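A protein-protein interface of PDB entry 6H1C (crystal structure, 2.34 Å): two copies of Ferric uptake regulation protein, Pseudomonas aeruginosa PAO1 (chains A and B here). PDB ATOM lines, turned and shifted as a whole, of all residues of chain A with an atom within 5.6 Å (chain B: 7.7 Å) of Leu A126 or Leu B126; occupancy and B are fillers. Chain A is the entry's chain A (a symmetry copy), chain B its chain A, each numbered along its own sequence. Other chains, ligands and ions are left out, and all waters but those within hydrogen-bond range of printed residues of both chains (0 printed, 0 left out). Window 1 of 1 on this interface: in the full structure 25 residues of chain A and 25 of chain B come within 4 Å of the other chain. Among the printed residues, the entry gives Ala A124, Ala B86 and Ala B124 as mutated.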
ATOM      1  N   HIS A  87     -11.064   0.412   0.445  1.00  0.00           N
ATOM      2  CA  HIS A  87     -12.428   0.039   0.792  1.00  0.00           C
ATOM      3  C   HIS A  87     -12.928  -1.186   0.044  1.00  0.00           C
ATOM      4  O   HIS A  87     -14.082  -1.576   0.239  1.00  0.00           O
ATOM      5  CB  HIS A  87     -13.402   1.193   0.522  1.00  0.00           C
ATOM      6  CG  HIS A  87     -12.803   2.551   0.682  1.00  0.00           C
ATOM      7  ND1 HIS A  87     -12.930   3.292   1.839  1.00  0.00           N
ATOM      8  CD2 HIS A  87     -12.084   3.316  -0.178  1.00  0.00           C
ATOM      9  CE1 HIS A  87     -12.313   4.453   1.688  1.00  0.00           C
ATOM     10  NE2 HIS A  87     -11.786   4.492   0.474  1.00  0.00           N
ATOM     11  N   ASP A  88     -12.107  -1.800  -0.803  1.00  0.00           N
ATOM     12  CA  ASP A  88     -12.493  -2.965  -1.596  1.00  0.00           C
ATOM     13  C   ASP A  88     -11.456  -4.061  -1.370  1.00  0.00           C
ATOM     14  O   ASP A  88     -10.295  -3.898  -1.757  1.00  0.00           O
ATOM     15  CB  ASP A  88     -12.595  -2.617  -3.087  1.00  0.00           C
ATOM     16  CG  ASP A  88     -13.840  -1.838  -3.428  1.00  0.00           C
ATOM     17  OD1 ASP A  88     -14.885  -2.477  -3.639  1.00  0.00           O
ATOM     18  OD2 ASP A  88     -13.789  -0.591  -3.494  1.00  0.00           O
ATOM     19  N   HIS A  89     -11.868  -5.170  -0.748  1.00  0.00           N
ATOM     20  CA  HIS A  89     -10.958  -6.253  -0.398  1.00  0.00           C
ATOM     21  C   HIS A  89     -11.627  -7.597  -0.633  1.00  0.00           C
ATOM     22  O   HIS A  89     -12.807  -7.761  -0.332  1.00  0.00           O
ATOM     23  CB  HIS A  89     -10.513  -6.176   1.085  1.00  0.00           C
ATOM     24  CG  HIS A  89      -9.609  -5.025   1.393  1.00  0.00           C
ATOM     25  ND1 HIS A  89     -10.078  -3.797   1.798  1.00  0.00           N
ATOM     26  CD2 HIS A  89      -8.260  -4.916   1.355  1.00  0.00           C
ATOM     27  CE1 HIS A  89      -9.060  -2.985   2.009  1.00  0.00           C
ATOM     28  NE2 HIS A  89      -7.944  -3.637   1.739  1.00  0.00           N
ATOM     29  N   PHE A 101      -8.875  -5.215  -4.530  1.00  0.00           N
ATOM     30  CA  PHE A 101      -9.285  -5.172  -5.921  1.00  0.00           C
ATOM     31  C   PHE A 101     -10.025  -3.868  -6.168  1.00  0.00           C
ATOM     32  O   PHE A 101     -10.450  -3.174  -5.239  1.00  0.00           O
ATOM     33  CB  PHE A 101     -10.169  -6.361  -6.308  1.00  0.00           C
ATOM     34  CG  PHE A 101     -11.509  -6.330  -5.667  1.00  0.00           C
ATOM     35  CD1 PHE A 101     -11.684  -6.807  -4.384  1.00  0.00           C
ATOM     36  CD2 PHE A 101     -12.592  -5.791  -6.330  1.00  0.00           C
ATOM     37  CE1 PHE A 101     -12.916  -6.764  -3.777  1.00  0.00           C
ATOM     38  CE2 PHE A 101     -13.826  -5.749  -5.729  1.00  0.00           C
ATOM     39  CZ  PHE A 101     -13.982  -6.240  -4.443  1.00  0.00           C
ATOM     40  N   ILE A 106     -18.452  -2.310 -10.853  1.00  0.00           N
ATOM     41  CA  ILE A 106     -18.972  -2.285  -9.485  1.00  0.00           C
ATOM     42  C   ILE A 106     -19.046  -0.860  -8.973  1.00  0.00           C
ATOM     43  O   ILE A 106     -20.068  -0.425  -8.435  1.00  0.00           O
ATOM     44  CB  ILE A 106     -18.107  -3.156  -8.562  1.00  0.00           C
ATOM     45  CG1 ILE A 106     -18.586  -4.600  -8.597  1.00  0.00           C
ATOM     46  CG2 ILE A 106     -18.106  -2.598  -7.148  1.00  0.00           C
ATOM     47  CD1 ILE A 106     -20.031  -4.753  -8.251  1.00  0.00           C
ATOM     48  N   GLN A 110     -22.580   1.192  -7.947  1.00  0.00           N
ATOM     49  CA  GLN A 110     -22.817   1.720  -6.603  1.00  0.00           C
ATOM     50  C   GLN A 110     -23.358   3.139  -6.660  1.00  0.00           C
ATOM     51  O   GLN A 110     -24.272   3.498  -5.911  1.00  0.00           O
ATOM     52  CB  GLN A 110     -21.534   1.709  -5.769  1.00  0.00           C
ATOM     53  CG  GLN A 110     -21.011   0.356  -5.349  1.00  0.00           C
ATOM     54  CD  GLN A 110     -19.666   0.466  -4.634  1.00  0.00           C
ATOM     55  OE1 GLN A 110     -19.034   1.529  -4.630  1.00  0.00           O
ATOM     56  NE2 GLN A 110     -19.229  -0.625  -4.027  1.00  0.00           N
ATOM     57  N   ALA A 124     -18.265   3.776   0.575  1.00  0.00           N
ATOM     58  CA  ALA A 124     -18.751   2.433   0.307  1.00  0.00           C
ATOM     59  C   ALA A 124     -17.709   1.436   0.794  1.00  0.00           C
ATOM     60  O   ALA A 124     -16.510   1.708   0.747  1.00  0.00           O
ATOM     61  CB  ALA A 124     -19.029   2.222  -1.190  1.00  0.00           C
ATOM     62  N   ASN A 125     -18.169   0.283   1.270  1.00  0.00           N
ATOM     63  CA  ASN A 125     -17.250  -0.775   1.661  1.00  0.00           C
ATOM     64  C   ASN A 125     -17.723  -2.111   1.129  1.00  0.00           C
ATOM     65  O   ASN A 125     -18.888  -2.482   1.314  1.00  0.00           O
ATOM     66  CB  ASN A 125     -17.092  -0.842   3.168  1.00  0.00           C
ATOM     67  CG  ASN A 125     -16.246   0.275   3.681  1.00  0.00           C
ATOM     68  OD1 ASN A 125     -15.320   0.723   3.001  1.00  0.00           O
ATOM     69  ND2 ASN A 125     -16.557   0.756   4.875  1.00  0.00           N
ATOM     70  N   LEU A 126     -16.810  -2.823   0.478  1.00  0.00           N
ATOM     71  CA  LEU A 126     -17.092  -4.123  -0.105  1.00  0.00           C
ATOM     72  C   LEU A 126     -16.089  -5.135   0.433  1.00  0.00           C
ATOM     73  O   LEU A 126     -14.883  -4.902   0.394  1.00  0.00           O
ATOM     74  CB  LEU A 126     -17.026  -4.033  -1.632  1.00  0.00           C
ATOM     75  CG  LEU A 126     -17.483  -5.248  -2.440  1.00  0.00           C
ATOM     76  CD1 LEU A 126     -18.852  -5.695  -1.981  1.00  0.00           C
ATOM     77  CD2 LEU A 126     -17.493  -4.951  -3.919  1.00  0.00           C
ATOM     78  N   VAL A 127     -16.567  -6.251   0.949  1.00  0.00           N
ATOM     79  CA  VAL A 127     -15.660  -7.315   1.357  1.00  0.00           C
ATOM     80  C   VAL A 127     -16.188  -8.620   0.801  1.00  0.00           C
ATOM     81  O   VAL A 127     -17.357  -8.959   1.015  1.00  0.00           O
ATOM     82  CB  VAL A 127     -15.494  -7.398   2.881  1.00  0.00           C
ATOM     83  CG1 VAL A 127     -14.630  -8.605   3.241  1.00  0.00           C
ATOM     84  CG2 VAL A 127     -14.858  -6.112   3.397  1.00  0.00           C
ATOM     85  N   LEU A 128     -15.332  -9.334   0.067  1.00  0.00           N
ATOM     86  CA  LEU A 128     -15.674 -10.608  -0.552  1.00  0.00           C
ATOM     87  C   LEU A 128     -14.891 -11.703   0.157  1.00  0.00           C
ATOM     88  O   LEU A 128     -13.669 -11.756   0.052  1.00  0.00           O
ATOM     89  CB  LEU A 128     -15.357 -10.590  -2.042  1.00  0.00           C
ATOM     90  CG  LEU A 128     -15.963  -9.475  -2.871  1.00  0.00           C
ATOM     91  CD1 LEU A 128     -15.597  -9.664  -4.332  1.00  0.00           C
ATOM     92  CD2 LEU A 128     -17.471  -9.441  -2.687  1.00  0.00           C
ATOM     93  N   HIS B  70     -23.885  -6.601  12.634  1.00  0.00           N
ATOM     94  CA  HIS B  70     -23.339  -5.399  12.025  1.00  0.00           C
ATOM     95  C   HIS B  70     -23.113  -4.353  13.103  1.00  0.00           C
ATOM     96  O   HIS B  70     -23.692  -4.423  14.184  1.00  0.00           O
ATOM     97  CB  HIS B  70     -24.264  -4.800  10.950  1.00  0.00           C
ATOM     98  CG  HIS B  70     -24.655  -5.754   9.864  1.00  0.00           C
ATOM     99  ND1 HIS B  70     -23.758  -6.245   8.939  1.00  0.00           N
ATOM    100  CD2 HIS B  70     -25.858  -6.278   9.531  1.00  0.00           C
ATOM    101  CE1 HIS B  70     -24.387  -7.039   8.096  1.00  0.00           C
ATOM    102  NE2 HIS B  70     -25.662  -7.074   8.431  1.00  0.00           N
ATOM    103  N   PHE B  72     -23.427  -0.443  12.465  1.00  0.00           N
ATOM    104  CA  PHE B  72     -23.635   0.514  11.381  1.00  0.00           C
ATOM    105  C   PHE B  72     -23.187   1.906  11.780  1.00  0.00           C
ATOM    106  O   PHE B  72     -22.490   2.579  11.013  1.00  0.00           O
ATOM    107  CB  PHE B  72     -25.096   0.537  10.937  1.00  0.00           C
ATOM    108  CG  PHE B  72     -25.533  -0.712  10.229  1.00  0.00           C
ATOM    109  CD1 PHE B  72     -24.924  -1.107   9.061  1.00  0.00           C
ATOM    110  CD2 PHE B  72     -26.560  -1.474  10.719  1.00  0.00           C
ATOM    111  CE1 PHE B  72     -25.330  -2.239   8.411  1.00  0.00           C
ATOM    112  CE2 PHE B  72     -26.958  -2.605  10.068  1.00  0.00           C
ATOM    113  CZ  PHE B  72     -26.338  -2.988   8.915  1.00  0.00           C
ATOM    114  N   ALA B  86     -29.490  -9.562   4.241  1.00  0.00           N
ATOM    115  CA  ALA B  86     -28.765  -9.228   5.456  1.00  0.00           C
ATOM    116  C   ALA B  86     -27.317  -8.805   5.229  1.00  0.00           C
ATOM    117  O   ALA B  86     -26.618  -8.558   6.212  1.00  0.00           O
ATOM    118  CB  ALA B  86     -28.787 -10.421   6.410  1.00  0.00           C
ATOM    119  N   HIS B  87     -26.841  -8.717   3.982  1.00  0.00           N
ATOM    120  CA  HIS B  87     -25.461  -8.346   3.703  1.00  0.00           C
ATOM    121  C   HIS B  87     -25.334  -7.103   2.839  1.00  0.00           C
ATOM    122  O   HIS B  87     -24.208  -6.712   2.517  1.00  0.00           O
ATOM    123  CB  HIS B  87     -24.710  -9.489   3.011  1.00  0.00           C
ATOM    124  CG  HIS B  87     -25.185 -10.853   3.389  1.00  0.00           C
ATOM    125  ND1 HIS B  87     -24.568 -11.617   4.356  1.00  0.00           N
ATOM    126  CD2 HIS B  87     -26.212 -11.604   2.914  1.00  0.00           C
ATOM    127  CE1 HIS B  87     -25.194 -12.779   4.466  1.00  0.00           C
ATOM    128  NE2 HIS B  87     -26.200 -12.794   3.606  1.00  0.00           N
ATOM    129  N   ASP B  88     -26.440  -6.476   2.450  1.00  0.00           N
ATOM    130  CA  ASP B  88     -26.434  -5.292   1.593  1.00  0.00           C
ATOM    131  C   ASP B  88     -27.262  -4.206   2.274  1.00  0.00           C
ATOM    132  O   ASP B  88     -28.476  -4.366   2.431  1.00  0.00           O
ATOM    133  CB  ASP B  88     -26.997  -5.608   0.201  1.00  0.00           C
ATOM    134  CG  ASP B  88     -26.031  -6.373  -0.667  1.00  0.00           C
ATOM    135  OD1 ASP B  88     -25.181  -5.724  -1.302  1.00  0.00           O
ATOM    136  OD2 ASP B  88     -26.112  -7.618  -0.731  1.00  0.00           O
ATOM    137  N   HIS B  89     -26.614  -3.108   2.675  1.00  0.00           N
ATOM    138  CA  HIS B  89     -27.273  -2.038   3.411  1.00  0.00           C
ATOM    139  C   HIS B  89     -26.768  -0.686   2.935  1.00  0.00           C
ATOM    140  O   HIS B  89     -25.575  -0.522   2.693  1.00  0.00           O
ATOM    141  CB  HIS B  89     -27.025  -2.148   4.937  1.00  0.00           C
ATOM    142  CG  HIS B  89     -27.708  -3.309   5.586  1.00  0.00           C
ATOM    143  ND1 HIS B  89     -27.115  -4.543   5.718  1.00  0.00           N
ATOM    144  CD2 HIS B  89     -28.938  -3.424   6.140  1.00  0.00           C
ATOM    145  CE1 HIS B  89     -27.942  -5.364   6.336  1.00  0.00           C
ATOM    146  NE2 HIS B  89     -29.061  -4.712   6.596  1.00  0.00           N
ATOM    147  N   MET B  90     -27.676   0.276   2.811  1.00  0.00           N
ATOM    148  CA  MET B  90     -27.339   1.690   2.818  1.00  0.00           C
ATOM    149  C   MET B  90     -27.552   2.226   4.226  1.00  0.00           C
ATOM    150  O   MET B  90     -28.362   1.699   4.988  1.00  0.00           O
ATOM    151  CB  MET B  90     -28.202   2.516   1.864  1.00  0.00           C
ATOM    152  CG  MET B  90     -28.183   2.138   0.397  1.00  0.00           C
ATOM    153  SD  MET B  90     -29.341   3.200  -0.525  1.00  0.00           S
ATOM    154  CE  MET B  90     -28.716   4.813  -0.122  1.00  0.00           C
ATOM    155  N   VAL B  91     -26.835   3.292   4.553  1.00  0.00           N
ATOM    156  CA  VAL B  91     -26.759   3.777   5.915  1.00  0.00           C
ATOM    157  C   VAL B  91     -26.599   5.284   5.871  1.00  0.00           C
ATOM    158  O   VAL B  91     -25.612   5.791   5.326  1.00  0.00           O
ATOM    159  CB  VAL B  91     -25.597   3.115   6.675  1.00  0.00           C
ATOM    160  CG1 VAL B  91     -25.364   3.818   7.998  1.00  0.00           C
ATOM    161  CG2 VAL B  91     -25.871   1.620   6.866  1.00  0.00           C
ATOM    162  N   ILE B  99     -31.086   0.989   5.568  1.00  0.00           N
ATOM    163  CA  ILE B  99     -32.013   0.557   4.521  1.00  0.00           C
ATOM    164  C   ILE B  99     -31.390  -0.586   3.753  1.00  0.00           C
ATOM    165  O   ILE B  99     -30.301  -0.438   3.191  1.00  0.00           O
ATOM    166  CB  ILE B  99     -32.367   1.695   3.545  1.00  0.00           C
ATOM    167  CG1 ILE B  99     -33.012   2.871   4.276  1.00  0.00           C
ATOM    168  CG2 ILE B  99     -33.259   1.170   2.428  1.00  0.00           C
ATOM    169  CD1 ILE B  99     -33.274   4.055   3.383  1.00  0.00           C
ATOM    170  N   PHE B 101     -30.960  -2.997   0.587  1.00  0.00           N
ATOM    171  CA  PHE B 101     -31.201  -3.009  -0.843  1.00  0.00           C
ATOM    172  C   PHE B 101     -30.651  -4.305  -1.417  1.00  0.00           C
ATOM    173  O   PHE B 101     -29.865  -5.015  -0.783  1.00  0.00           O
ATOM    174  CB  PHE B 101     -30.570  -1.809  -1.553  1.00  0.00           C
ATOM    175  CG  PHE B 101     -29.085  -1.847  -1.565  1.00  0.00           C
ATOM    176  CD1 PHE B 101     -28.363  -1.395  -0.477  1.00  0.00           C
ATOM    177  CD2 PHE B 101     -28.404  -2.366  -2.646  1.00  0.00           C
ATOM    178  CE1 PHE B 101     -26.990  -1.446  -0.473  1.00  0.00           C
ATOM    179  CE2 PHE B 101     -27.032  -2.415  -2.647  1.00  0.00           C
ATOM    180  CZ  PHE B 101     -26.325  -1.950  -1.549  1.00  0.00           C
ATOM    181  N   ASP B 103     -29.477  -5.567  -5.504  1.00  0.00           N
ATOM    182  CA  ASP B 103     -29.292  -5.175  -6.892  1.00  0.00           C
ATOM    183  C   ASP B 103     -28.635  -6.341  -7.604  1.00  0.00           C
ATOM    184  O   ASP B 103     -27.540  -6.765  -7.217  1.00  0.00           O
ATOM    185  CB  ASP B 103     -28.436  -3.907  -6.998  1.00  0.00           C
ATOM    186  CG  ASP B 103     -28.235  -3.436  -8.443  1.00  0.00           C
ATOM    187  OD1 ASP B 103     -29.111  -2.724  -8.994  1.00  0.00           O
ATOM    188  OD2 ASP B 103     -27.181  -3.760  -9.027  1.00  0.00           O
ATOM    189  N   ILE B 106     -25.133  -5.722  -9.350  1.00  0.00           N
ATOM    190  CA  ILE B 106     -24.067  -5.773  -8.349  1.00  0.00           C
ATOM    191  C   ILE B 106     -23.783  -7.209  -7.951  1.00  0.00           C
ATOM    192  O   ILE B 106     -22.631  -7.650  -7.925  1.00  0.00           O
ATOM    193  CB  ILE B 106     -24.436  -4.926  -7.122  1.00  0.00           C
ATOM    194  CG1 ILE B 106     -24.014  -3.480  -7.333  1.00  0.00           C
ATOM    195  CG2 ILE B 106     -23.820  -5.514  -5.862  1.00  0.00           C
ATOM    196  CD1 ILE B 106     -22.563  -3.326  -7.652  1.00  0.00           C
ATOM    197  N   GLU B 107     -24.835  -7.963  -7.635  1.00  0.00           N
ATOM    198  CA  GLU B 107     -24.620  -9.333  -7.183  1.00  0.00           C
ATOM    199  C   GLU B 107     -24.016 -10.201  -8.283  1.00  0.00           C
ATOM    200  O   GLU B 107     -23.316 -11.180  -7.993  1.00  0.00           O
ATOM    201  CB  GLU B 107     -25.932  -9.938  -6.673  1.00  0.00           C
ATOM    202  CG  GLU B 107     -26.542  -9.220  -5.450  1.00  0.00           C
ATOM    203  CD  GLU B 107     -25.785  -9.464  -4.136  1.00  0.00           C
ATOM    204  OE1 GLU B 107     -25.275 -10.586  -3.931  1.00  0.00           O
ATOM    205  OE2 GLU B 107     -25.710  -8.528  -3.302  1.00  0.00           O
ATOM    206  N   ARG B 109     -21.898  -8.998 -10.831  1.00  0.00           N
ATOM    207  CA  ARG B 109     -20.512  -8.567 -10.950  1.00  0.00           C
ATOM    208  C   ARG B 109     -19.637  -9.150  -9.844  1.00  0.00           C
ATOM    209  O   ARG B 109     -18.475  -9.492 -10.086  1.00  0.00           O
ATOM    210  CB  ARG B 109     -20.460  -7.045 -10.933  1.00  0.00           C
ATOM    211  CG  ARG B 109     -19.178  -6.491 -11.451  1.00  0.00           C
ATOM    212  CD  ARG B 109     -18.848  -7.125 -12.773  1.00  0.00           C
ATOM    213  NE  ARG B 109     -17.537  -6.694 -13.228  1.00  0.00           N
ATOM    214  CZ  ARG B 109     -16.788  -7.367 -14.091  1.00  0.00           C
ATOM    215  NH1 ARG B 109     -17.226  -8.513 -14.597  1.00  0.00           N
ATOM    216  NH2 ARG B 109     -15.598  -6.894 -14.434  1.00  0.00           N
ATOM    217  N   GLN B 110     -20.167  -9.265  -8.619  1.00  0.00           N
ATOM    218  CA  GLN B 110     -19.367  -9.820  -7.526  1.00  0.00           C
ATOM    219  C   GLN B 110     -18.913 -11.235  -7.845  1.00  0.00           C
ATOM    220  O   GLN B 110     -17.765 -11.605  -7.580  1.00  0.00           O
ATOM    221  CB  GLN B 110     -20.156  -9.832  -6.215  1.00  0.00           C
ATOM    222  CG  GLN B 110     -20.435  -8.491  -5.580  1.00  0.00           C
ATOM    223  CD  GLN B 110     -21.332  -8.623  -4.351  1.00  0.00           C
ATOM    224  OE1 GLN B 110     -21.904  -9.689  -4.093  1.00  0.00           O
ATOM    225  NE2 GLN B 110     -21.454  -7.547  -3.591  1.00  0.00           N
ATOM    226  N   ILE B 113     -16.163 -11.152 -10.650  1.00  0.00           N
ATOM    227  CA  ILE B 113     -14.865 -10.740 -10.116  1.00  0.00           C
ATOM    228  C   ILE B 113     -14.158 -11.925  -9.484  1.00  0.00           C
ATOM    229  O   ILE B 113     -12.982 -12.193  -9.751  1.00  0.00           O
ATOM    230  CB  ILE B 113     -15.042  -9.610  -9.094  1.00  0.00           C
ATOM    231  CG1 ILE B 113     -15.371  -8.305  -9.790  1.00  0.00           C
ATOM    232  CG2 ILE B 113     -13.800  -9.446  -8.289  1.00  0.00           C
ATOM    233  CD1 ILE B 113     -15.694  -7.228  -8.814  1.00  0.00           C
ATOM    234  N   ASP B 123     -19.105 -15.382   0.911  1.00  0.00           N
ATOM    235  CA  ASP B 123     -19.961 -14.350   1.466  1.00  0.00           C
ATOM    236  C   ASP B 123     -19.422 -13.000   1.031  1.00  0.00           C
ATOM    237  O   ASP B 123     -18.218 -12.833   0.839  1.00  0.00           O
ATOM    238  CB  ASP B 123     -20.020 -14.419   2.994  1.00  0.00           C
ATOM    239  CG  ASP B 123     -21.283 -13.793   3.545  1.00  0.00           C
ATOM    240  OD1 ASP B 123     -21.384 -12.542   3.575  1.00  0.00           O
ATOM    241  OD2 ASP B 123     -22.189 -14.561   3.933  1.00  0.00           O
ATOM    242  N   ALA B 124     -20.327 -12.049   0.875  1.00  0.00           N
ATOM    243  CA  ALA B 124     -20.001 -10.698   0.449  1.00  0.00           C
ATOM    244  C   ALA B 124     -20.720  -9.716   1.363  1.00  0.00           C
ATOM    245  O   ALA B 124     -21.820  -9.993   1.841  1.00  0.00           O
ATOM    246  CB  ALA B 124     -20.406 -10.454  -1.014  1.00  0.00           C
ATOM    247  N   ASN B 125     -20.092  -8.571   1.616  1.00  0.00           N
ATOM    248  CA  ASN B 125     -20.742  -7.527   2.391  1.00  0.00           C
ATOM    249  C   ASN B 125     -20.543  -6.178   1.734  1.00  0.00           C
ATOM    250  O   ASN B 125     -19.413  -5.805   1.398  1.00  0.00           O
ATOM    251  CB  ASN B 125     -20.224  -7.492   3.816  1.00  0.00           C
ATOM    252  CG  ASN B 125     -20.765  -8.624   4.624  1.00  0.00           C
ATOM    253  OD1 ASN B 125     -21.897  -9.062   4.409  1.00  0.00           O
ATOM    254  ND2 ASN B 125     -19.965  -9.128   5.551  1.00  0.00           N
ATOM    255  N   LEU B 126     -21.645  -5.457   1.564  1.00  0.00           N
ATOM    256  CA  LEU B 126     -21.641  -4.143   0.944  1.00  0.00           C
ATOM    257  C   LEU B 126     -22.303  -3.147   1.888  1.00  0.00           C
ATOM    258  O   LEU B 126     -23.405  -3.386   2.375  1.00  0.00           O
ATOM    259  CB  LEU B 126     -22.369  -4.201  -0.402  1.00  0.00           C
ATOM    260  CG  LEU B 126     -22.307  -2.967  -1.302  1.00  0.00           C
ATOM    261  CD1 LEU B 126     -20.872  -2.524  -1.479  1.00  0.00           C
ATOM    262  CD2 LEU B 126     -22.946  -3.232  -2.642  1.00  0.00           C
ATOM    263  N   VAL B 127     -21.642  -2.041   2.166  1.00  0.00           N
ATOM    264  CA  VAL B 127     -22.273  -0.989   2.952  1.00  0.00           C
ATOM    265  C   VAL B 127     -22.035   0.329   2.249  1.00  0.00           C
ATOM    266  O   VAL B 127     -20.889   0.670   1.936  1.00  0.00           O
ATOM    267  CB  VAL B 127     -21.754  -0.940   4.397  1.00  0.00           C
ATOM    268  CG1 VAL B 127     -22.367   0.255   5.124  1.00  0.00           C
ATOM    269  CG2 VAL B 127     -22.107  -2.239   5.111  1.00  0.00           C
ATOM    270  N   LEU B 128     -23.123   1.055   1.979  1.00  0.00           N
ATOM    271  CA  LEU B 128     -23.080   2.343   1.300  1.00  0.00           C
ATOM    272  C   LEU B 128     -23.468   3.419   2.303  1.00  0.00           C
ATOM    273  O   LEU B 128     -24.612   3.469   2.745  1.00  0.00           O
ATOM    274  CB  LEU B 128     -24.017   2.355   0.099  1.00  0.00           C
ATOM    275  CG  LEU B 128     -23.841   1.261  -0.935  1.00  0.00           C
ATOM    276  CD1 LEU B 128     -24.809   1.479  -2.084  1.00  0.00           C
ATOM    277  CD2 LEU B 128     -22.405   1.230  -1.431  1.00  0.00           C
ATOM    278  N   TYR B 129     -22.516   4.260   2.671  1.00  0.00           N
ATOM    279  CA  TYR B 129     -22.773   5.398   3.545  1.00  0.00           C
ATOM    280  C   TYR B 129     -23.173   6.580   2.682  1.00  0.00           C
ATOM    281  O   TYR B 129     -22.426   6.980   1.783  1.00  0.00           O
ATOM    282  CB  TYR B 129     -21.546   5.737   4.385  1.00  0.00           C
ATOM    283  CG  TYR B 129     -21.144   4.593   5.272  1.00  0.00           C
ATOM    284  CD1 TYR B 129     -21.829   4.338   6.454  1.00  0.00           C
ATOM    285  CD2 TYR B 129     -20.106   3.748   4.925  1.00  0.00           C
ATOM    286  CE1 TYR B 129     -21.483   3.279   7.282  1.00  0.00           C
ATOM    287  CE2 TYR B 129     -19.746   2.700   5.747  1.00  0.00           C
ATOM    288  CZ  TYR B 129     -20.444   2.467   6.923  1.00  0.00           C
ATOM    289  OH  TYR B 129     -20.113   1.417   7.748  1.00  0.00           O
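The backbone NH (N) of Asn A125 sits at hydrogen-bond distance from the backbone carbonyl oxygen (O) of Val B127 (2.8 Å). The backbone carbonyl oxygen (O) of Asn A125 sits close to the backbone carbonyl oxygen (O) of Asn B125 (3.4 Å). O of Val A127 lies within hydrogen-bond range of N of Asn B125.
The backbone carbonyl oxygen of Leu B126 lies within hydrogen-bond range of the backbone NH of His B89. The backbone carbonyl oxygen (O) of His A87 sits at hydrogen-bond distance from the backbone NH (N) of Leu A126 (3.0 Å). The backbone carbonyl oxygen (O) of Leu A126 lies within hydrogen-bond range of the backbone NH (N) of His A89 (3.2 Å). The backbone NH of Leu B128 is in hydrogen-bond range of the backbone carbonyl oxygen of His B89, at 3.0 Å. The backbone NH of Val B91 is in hydrogen-bond range of the backbone carbonyl oxygen of Leu B128 (2.9 Å). OE1 of Glu B107 lies close to OE1 of Gln B110.
Among the printed residues, merely in contact across the chains: Ile A106 with Ile B106 (3.0 Å), Ala A124 with Val B127 (3.2 Å), Val A127 with Ala B124 (3.2 Å), Asn A125 with Leu B126 (3.2 Å), Leu A126 with Asn B125 (3.2 Å), Ile A106 with Arg B109 (3.5 Å), Leu A128 with Ala B124 (3.5 Å), Ala A124 with Leu B128 (3.5 Å), Leu A126 with Gln B110 (3.6 Å), Gln A110 with Leu B126 (3.6 Å), Leu A128 with Asp B123 (3.6 Å), Leu A126 with Leu B126 (3.8 Å), Asn A125 with Tyr B129 (3.8 Å), Phe A101 with Ile B113 (3.9 Å), Ile A106 with Ile B113 (3.9 Å) and Val A127 with Asp B123 (3.97 Å).
Of the printed residues of chain B, Ile A106 touches Ile B106, Arg B109 and Ile B113. Printed residues of chain B within 4 Å of Gln A110: Leu B126 (3.6 Å). Printed residues of chain B within 4 Å of Asn A125: Asn B125 (3.4 Å), Leu B126 (3.2 Å), Val B127 (2.8 Å) and Tyr B129 (3.8 Å). Leu A126 touches just these residues of chain B: Gln B110, Asn B125 and Leu B126. Of the printed residues of chain B, Val A127 touches Asp B123, Ala B124 and Asn B125. Leu B126 touches just these residues of chain A: Gln A110 (3.6 Å), Asn A125 (3.2 Å) and Leu A126 (3.8 Å). The nearest residue of chain A that does not touch Leu B126 is Ala A124 (5.1 Å).
Of the 23 printed residues of chain B, 11 touch a printed residue of chain A. Hydrophobic or aromatic side chains of chain B that line the printed part of chain A: Ile B106, Ile B113, Ala B124, Leu B126, Leu B128 and Tyr B129. Printed residues of chain A that touch a printed residue of chain B: Phe A101, Ile A106, Gln A110, Ala A124, Asn A125, Leu A126, Val A127 and Leu A128. Hydrophobic or aromatic side chains of chain A that line the printed part of chain B: Phe A101, Ile A106, Ala A124, Leu A126 and Leu A128.
Ile A106 touches its own counterpart, Ile B106. Ala A124 touches Val B127, and with the chains exchanged Val A127 touches Ala B124. Ala A124 touches Leu B128, and with the chains exchanged Leu A128 touches Ala B124. Asn A125 touches Val B127, and with the chains exchanged Val A127 touches Asn B125.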
